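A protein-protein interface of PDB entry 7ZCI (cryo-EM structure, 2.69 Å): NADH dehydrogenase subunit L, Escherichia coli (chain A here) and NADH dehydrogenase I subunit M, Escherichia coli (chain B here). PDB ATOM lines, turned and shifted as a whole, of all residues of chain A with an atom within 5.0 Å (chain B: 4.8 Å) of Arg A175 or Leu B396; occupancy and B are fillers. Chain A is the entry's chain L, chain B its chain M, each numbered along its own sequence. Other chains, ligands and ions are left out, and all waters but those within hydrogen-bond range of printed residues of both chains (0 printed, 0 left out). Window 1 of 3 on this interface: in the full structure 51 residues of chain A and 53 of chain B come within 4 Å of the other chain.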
ATOM      1  N   GLU A 144     -27.006  23.688  14.851  1.00  0.00           N
ATOM      2  CA  GLU A 144     -27.185  23.997  13.440  1.00  0.00           C
ATOM      3  C   GLU A 144     -28.536  24.639  13.174  1.00  0.00           C
ATOM      4  O   GLU A 144     -28.669  25.461  12.260  1.00  0.00           O
ATOM      5  CB  GLU A 144     -27.036  22.727  12.623  1.00  0.00           C
ATOM      6  CG  GLU A 144     -25.651  22.130  12.566  1.00  0.00           C
ATOM      7  CD  GLU A 144     -24.709  22.899  11.672  1.00  0.00           C
ATOM      8  OE1 GLU A 144     -23.493  22.635  11.735  1.00  0.00           O
ATOM      9  OE2 GLU A 144     -25.177  23.750  10.887  1.00  0.00           O
ATOM     10  N   ALA A 170     -22.461  35.563   8.659  1.00  0.00           N
ATOM     11  CA  ALA A 170     -22.781  34.967   9.953  1.00  0.00           C
ATOM     12  C   ALA A 170     -22.881  33.453   9.855  1.00  0.00           C
ATOM     13  O   ALA A 170     -22.344  32.732  10.707  1.00  0.00           O
ATOM     14  CB  ALA A 170     -24.080  35.556  10.495  1.00  0.00           C
ATOM     15  N   PHE A 171     -23.525  32.955   8.797  1.00  0.00           N
ATOM     16  CA  PHE A 171     -23.661  31.514   8.625  1.00  0.00           C
ATOM     17  C   PHE A 171     -22.313  30.842   8.397  1.00  0.00           C
ATOM     18  O   PHE A 171     -22.064  29.763   8.936  1.00  0.00           O
ATOM     19  CB  PHE A 171     -24.615  31.201   7.477  1.00  0.00           C
ATOM     20  CG  PHE A 171     -25.143  29.797   7.502  1.00  0.00           C
ATOM     21  CD1 PHE A 171     -26.186  29.453   8.340  1.00  0.00           C
ATOM     22  CD2 PHE A 171     -24.580  28.815   6.710  1.00  0.00           C
ATOM     23  CE1 PHE A 171     -26.671  28.168   8.370  1.00  0.00           C
ATOM     24  CE2 PHE A 171     -25.060  27.530   6.736  1.00  0.00           C
ATOM     25  CZ  PHE A 171     -26.107  27.206   7.568  1.00  0.00           C
ATOM     26  N   VAL A 172     -21.418  31.471   7.631  1.00  0.00           N
ATOM     27  CA  VAL A 172     -20.135  30.838   7.333  1.00  0.00           C
ATOM     28  C   VAL A 172     -19.239  30.797   8.572  1.00  0.00           C
ATOM     29  O   VAL A 172     -18.602  29.770   8.853  1.00  0.00           O
ATOM     30  CB  VAL A 172     -19.455  31.542   6.144  1.00  0.00           C
ATOM     31  CG1 VAL A 172     -17.993  31.162   6.049  1.00  0.00           C
ATOM     32  CG2 VAL A 172     -20.159  31.175   4.857  1.00  0.00           C
ATOM     33  N   VAL A 173     -19.180  31.892   9.340  1.00  0.00           N
ATOM     34  CA  VAL A 173     -18.364  31.870  10.557  1.00  0.00           C
ATOM     35  C   VAL A 173     -18.931  30.890  11.583  1.00  0.00           C
ATOM     36  O   VAL A 173     -18.181  30.133  12.225  1.00  0.00           O
ATOM     37  CB  VAL A 173     -18.201  33.285  11.143  1.00  0.00           C
ATOM     38  CG1 VAL A 173     -17.120  33.283  12.182  1.00  0.00           C
ATOM     39  CG2 VAL A 173     -17.759  34.238  10.071  1.00  0.00           C
ATOM     40  N   THR A 174     -20.262  30.852  11.733  1.00  0.00           N
ATOM     41  CA  THR A 174     -20.836  29.872  12.644  1.00  0.00           C
ATOM     42  C   THR A 174     -20.642  28.445  12.145  1.00  0.00           C
ATOM     43  O   THR A 174     -20.512  27.532  12.957  1.00  0.00           O
ATOM     44  CB  THR A 174     -22.315  30.161  12.879  1.00  0.00           C
ATOM     45  OG1 THR A 174     -22.974  30.341  11.624  1.00  0.00           O
ATOM     46  CG2 THR A 174     -22.476  31.411  13.718  1.00  0.00           C
ATOM     47  N   ARG A 175     -20.565  28.229  10.831  1.00  0.00           N
ATOM     48  CA  ARG A 175     -20.311  26.881  10.332  1.00  0.00           C
ATOM     49  C   ARG A 175     -18.866  26.454  10.530  1.00  0.00           C
ATOM     50  O   ARG A 175     -18.603  25.263  10.712  1.00  0.00           O
ATOM     51  CB  ARG A 175     -20.687  26.778   8.858  1.00  0.00           C
ATOM     52  CG  ARG A 175     -22.160  26.524   8.640  1.00  0.00           C
ATOM     53  CD  ARG A 175     -22.531  25.082   8.892  1.00  0.00           C
ATOM     54  NE  ARG A 175     -22.445  24.295   7.671  1.00  0.00           N
ATOM     55  CZ  ARG A 175     -23.055  23.134   7.486  1.00  0.00           C
ATOM     56  NH1 ARG A 175     -23.809  22.593   8.427  1.00  0.00           N
ATOM     57  NH2 ARG A 175     -22.911  22.505   6.324  1.00  0.00           N
ATOM     58  N   VAL A 176     -17.923  27.397  10.502  1.00  0.00           N
ATOM     59  CA  VAL A 176     -16.552  27.071  10.896  1.00  0.00           C
ATOM     60  C   VAL A 176     -16.512  26.651  12.361  1.00  0.00           C
ATOM     61  O   VAL A 176     -15.872  25.647  12.729  1.00  0.00           O
ATOM     62  CB  VAL A 176     -15.614  28.259  10.618  1.00  0.00           C
ATOM     63  CG1 VAL A 176     -14.225  27.967  11.138  1.00  0.00           C
ATOM     64  CG2 VAL A 176     -15.560  28.553   9.136  1.00  0.00           C
ATOM     65  N   GLY A 177     -17.228  27.391  13.214  1.00  0.00           N
ATOM     66  CA  GLY A 177     -17.359  26.974  14.603  1.00  0.00           C
ATOM     67  C   GLY A 177     -18.012  25.610  14.751  1.00  0.00           C
ATOM     68  O   GLY A 177     -17.600  24.794  15.579  1.00  0.00           O
ATOM     69  N   ASP A 178     -19.014  25.330  13.923  1.00  0.00           N
ATOM     70  CA  ASP A 178     -19.718  24.058  14.000  1.00  0.00           C
ATOM     71  C   ASP A 178     -18.855  22.906  13.505  1.00  0.00           C
ATOM     72  O   ASP A 178     -19.020  21.770  13.953  1.00  0.00           O
ATOM     73  CB  ASP A 178     -21.011  24.147  13.203  1.00  0.00           C
ATOM     74  CG  ASP A 178     -22.108  24.831  13.975  1.00  0.00           C
ATOM     75  OD1 ASP A 178     -23.274  24.404  13.894  1.00  0.00           O
ATOM     76  OD2 ASP A 178     -21.802  25.808  14.685  1.00  0.00           O
ATOM     77  N   VAL A 179     -17.928  23.179  12.592  1.00  0.00           N
ATOM     78  CA  VAL A 179     -16.964  22.165  12.181  1.00  0.00           C
ATOM     79  C   VAL A 179     -15.988  21.861  13.311  1.00  0.00           C
ATOM     80  O   VAL A 179     -15.615  20.698  13.535  1.00  0.00           O
ATOM     81  CB  VAL A 179     -16.264  22.618  10.886  1.00  0.00           C
ATOM     82  CG1 VAL A 179     -14.842  22.124  10.799  1.00  0.00           C
ATOM     83  CG2 VAL A 179     -17.049  22.102   9.726  1.00  0.00           C
ATOM     84  N   ALA B 392     -31.745  23.572  -0.758  1.00  0.00           N
ATOM     85  CA  ALA B 392     -30.393  24.088  -0.566  1.00  0.00           C
ATOM     86  C   ALA B 392     -29.918  23.866   0.866  1.00  0.00           C
ATOM     87  O   ALA B 392     -28.749  23.543   1.098  1.00  0.00           O
ATOM     88  CB  ALA B 392     -30.336  25.566  -0.936  1.00  0.00           C
ATOM     89  N   VAL B 393     -30.820  24.036   1.835  1.00  0.00           N
ATOM     90  CA  VAL B 393     -30.547  23.682   3.225  1.00  0.00           C
ATOM     91  C   VAL B 393     -30.256  22.190   3.382  1.00  0.00           C
ATOM     92  O   VAL B 393     -29.377  21.800   4.159  1.00  0.00           O
ATOM     93  CB  VAL B 393     -31.733  24.164   4.084  1.00  0.00           C
ATOM     94  CG1 VAL B 393     -31.680  23.625   5.463  1.00  0.00           C
ATOM     95  CG2 VAL B 393     -31.677  25.668   4.203  1.00  0.00           C
ATOM     96  N   ALA B 394     -30.956  21.339   2.636  1.00  0.00           N
ATOM     97  CA  ALA B 394     -30.732  19.899   2.733  1.00  0.00           C
ATOM     98  C   ALA B 394     -29.382  19.505   2.144  1.00  0.00           C
ATOM     99  O   ALA B 394     -28.620  18.763   2.772  1.00  0.00           O
ATOM    100  CB  ALA B 394     -31.866  19.144   2.045  1.00  0.00           C
ATOM    101  N   THR B 395     -29.054  20.003   0.948  1.00  0.00           N
ATOM    102  CA  THR B 395     -27.751  19.697   0.360  1.00  0.00           C
ATOM    103  C   THR B 395     -26.615  20.410   1.070  1.00  0.00           C
ATOM    104  O   THR B 395     -25.451  20.062   0.851  1.00  0.00           O
ATOM    105  CB  THR B 395     -27.699  20.059  -1.129  1.00  0.00           C
ATOM    106  OG1 THR B 395     -26.377  19.833  -1.623  1.00  0.00           O
ATOM    107  CG2 THR B 395     -27.977  21.505  -1.338  1.00  0.00           C
ATOM    108  N   LEU B 396     -26.925  21.408   1.892  1.00  0.00           N
ATOM    109  CA  LEU B 396     -25.913  22.067   2.701  1.00  0.00           C
ATOM    110  C   LEU B 396     -25.377  21.139   3.784  1.00  0.00           C
ATOM    111  O   LEU B 396     -24.216  21.260   4.184  1.00  0.00           O
ATOM    112  CB  LEU B 396     -26.521  23.331   3.303  1.00  0.00           C
ATOM    113  CG  LEU B 396     -25.744  24.293   4.182  1.00  0.00           C
ATOM    114  CD1 LEU B 396     -26.174  25.694   3.811  1.00  0.00           C
ATOM    115  CD2 LEU B 396     -26.014  24.020   5.640  1.00  0.00           C
ATOM    116  N   GLY B 397     -26.201  20.211   4.261  1.00  0.00           N
ATOM    117  CA  GLY B 397     -25.798  19.298   5.310  1.00  0.00           C
ATOM    118  C   GLY B 397     -26.460  19.607   6.636  1.00  0.00           C
ATOM    119  O   GLY B 397     -25.877  19.379   7.698  1.00  0.00           O
ATOM    120  N   MET B 398     -27.677  20.121   6.583  1.00  0.00           N
ATOM    121  CA  MET B 398     -28.357  20.572   7.789  1.00  0.00           C
ATOM    122  C   MET B 398     -29.004  19.402   8.516  1.00  0.00           C
ATOM    123  O   MET B 398     -29.606  18.536   7.874  1.00  0.00           O
ATOM    124  CB  MET B 398     -29.402  21.620   7.457  1.00  0.00           C
ATOM    125  CG  MET B 398     -28.932  23.058   7.644  1.00  0.00           C
ATOM    126  SD  MET B 398     -28.351  23.433   9.293  1.00  0.00           S
ATOM    127  CE  MET B 398     -29.846  23.085  10.201  1.00  0.00           C
ATOM    128  N   LEU B 429     -17.506  20.401   4.332  1.00  0.00           N
ATOM    129  CA  LEU B 429     -18.871  20.807   4.709  1.00  0.00           C
ATOM    130  C   LEU B 429     -19.007  22.327   4.788  1.00  0.00           C
ATOM    131  O   LEU B 429     -20.054  22.889   4.423  1.00  0.00           O
ATOM    132  CB  LEU B 429     -19.320  20.215   6.052  1.00  0.00           C
ATOM    133  CG  LEU B 429     -19.748  18.793   6.418  1.00  0.00           C
ATOM    134  CD1 LEU B 429     -18.770  17.746   6.023  1.00  0.00           C
ATOM    135  CD2 LEU B 429     -20.011  18.724   7.914  1.00  0.00           C
ATOM    136  N   VAL B 430     -17.972  23.001   5.301  1.00  0.00           N
ATOM    137  CA  VAL B 430     -17.963  24.475   5.275  1.00  0.00           C
ATOM    138  C   VAL B 430     -18.098  24.995   3.844  1.00  0.00           C
ATOM    139  O   VAL B 430     -18.895  25.906   3.558  1.00  0.00           O
ATOM    140  CB  VAL B 430     -16.692  25.035   5.941  1.00  0.00           C
ATOM    141  CG1 VAL B 430     -16.584  26.533   5.709  1.00  0.00           C
ATOM    142  CG2 VAL B 430     -16.722  24.789   7.404  1.00  0.00           C
ATOM    143  N   ALA B 432     -19.427  23.454   1.343  1.00  0.00           N
ATOM    144  CA  ALA B 432     -20.773  23.134   0.878  1.00  0.00           C
ATOM    145  C   ALA B 432     -21.775  24.194   1.306  1.00  0.00           C
ATOM    146  O   ALA B 432     -22.639  24.609   0.515  1.00  0.00           O
ATOM    147  CB  ALA B 432     -21.197  21.766   1.403  1.00  0.00           C
ATOM    148  N   SER B 433     -21.668  24.643   2.558  1.00  0.00           N
ATOM    149  CA  SER B 433     -22.505  25.747   3.020  1.00  0.00           C
ATOM    150  C   SER B 433     -22.260  27.002   2.193  1.00  0.00           C
ATOM    151  O   SER B 433     -23.211  27.716   1.842  1.00  0.00           O
ATOM    152  CB  SER B 433     -22.247  26.023   4.499  1.00  0.00           C
ATOM    153  OG  SER B 433     -21.035  26.731   4.678  1.00  0.00           O
ATOM    154  N   SER B 436     -24.040  26.655  -1.219  1.00  0.00           N
ATOM    155  CA  SER B 436     -25.498  26.662  -1.094  1.00  0.00           C
ATOM    156  C   SER B 436     -26.027  28.070  -0.837  1.00  0.00           C
ATOM    157  O   SER B 436     -27.005  28.505  -1.467  1.00  0.00           O
ATOM    158  CB  SER B 436     -25.936  25.706   0.011  1.00  0.00           C
ATOM    159  OG  SER B 436     -25.657  24.366  -0.345  1.00  0.00           O
ATOM    160  N   LEU B 437     -25.377  28.811   0.070  1.00  0.00           N
ATOM    161  CA  LEU B 437     -25.790  30.193   0.289  1.00  0.00           C
ATOM    162  C   LEU B 437     -25.528  31.062  -0.933  1.00  0.00           C
ATOM    163  O   LEU B 437     -26.303  31.986  -1.199  1.00  0.00           O
ATOM    164  CB  LEU B 437     -25.087  30.796   1.502  1.00  0.00           C
ATOM    165  CG  LEU B 437     -25.099  30.058   2.835  1.00  0.00           C
ATOM    166  CD1 LEU B 437     -24.112  30.729   3.768  1.00  0.00           C
ATOM    167  CD2 LEU B 437     -26.487  30.000   3.436  1.00  0.00           C
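Leu B396 touches Phe A171.
Phe A171 touches Ser B433.
Leu B437 touches Phe A171.
NH1 of Arg A175 touches O of Gly B397, 3.9 Å away.
Arg A175 touches Val B430.
NE of Arg A175 touches CB of Ser B433, at 3.6 Å.
Val A179 touches Val B430.
O of Leu B396 lies within hydrogen-bond range of NH2 of Arg A175 (2.8 Å).
The guanidinium group (NH2) of Arg A175 sits at hydrogen-bond distance from the backbone carbonyl oxygen (O) of Leu B429, at 3.5 Å.
The side-chain sulfur of Met B398 lies close to the side-chain carboxylate of Glu A144 (3.6 Å).
Of chain B, only Leu B396 (2.8 Å), Gly B397 (3.9 Å), Leu B429 (3.5 Å), Val B430 (3.8 Å) and Ser B433 (3.6 Å) come within 4 Å of Arg A175.
Leu B396 touches just these residues of chain A: Phe A171 (3.6 Å) and Arg A175 (2.8 Å).
Of the printed residues of chain A, Met B398 touches Glu A144.
Printed residues of chain A within 4 Å of Ser B433: Phe A171 and Arg A175.
Of the printed residues of chain B, Val A179 touches Val B430.
Of the printed residues of chain B, Phe A171 touches Leu B396, Ser B433 and Leu B437.
Thr A174 touches none of the printed residues of chain B.
The nearest printed residue of chain A that does not touch Leu B396 is Glu A144 (5.3 Å).
The nearest printed residue of chain A that does not touch Leu B429 is Val A179 (4.7 Å).
Printed residues of chain A that touch a printed residue of chain B: Glu A144, Phe A171, Arg A175 and Val A179.
Hydrophobic or aromatic side chains of chain A that line the printed part of chain B: Phe A171 and Val A179.
Along chain A the printed residues that touch a printed residue of chain B span positions 144 to 179.
Of the 13 printed residues of chain B, 7 touch a printed residue of chain A.
Hydrophobic or aromatic side chains of chain B that line the printed part of chain A: Leu B396, Met B398, Val B430 and Leu B437.
Among the printed residues, no Asp or Glu carboxylate lies within 4 Å of a Lys or Arg side-chain nitrogen of the other chain.
The backbone NH (N) of Met B398 lies close to the backbone carbonyl oxygen (O) of Val B393, at 3.4 Å.
The backbone carbonyl oxygen (O) of Val B430 sits at hydrogen-bond distance from the side-chain hydroxyl (OG) of Ser B433 (2.6 Å).
OE2 of Glu A144 lies within salt-bridge range of NH1 of Arg A175 (3.0 Å).
O of Phe A171 is in hydrogen-bond range of OG1 of Thr A174.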
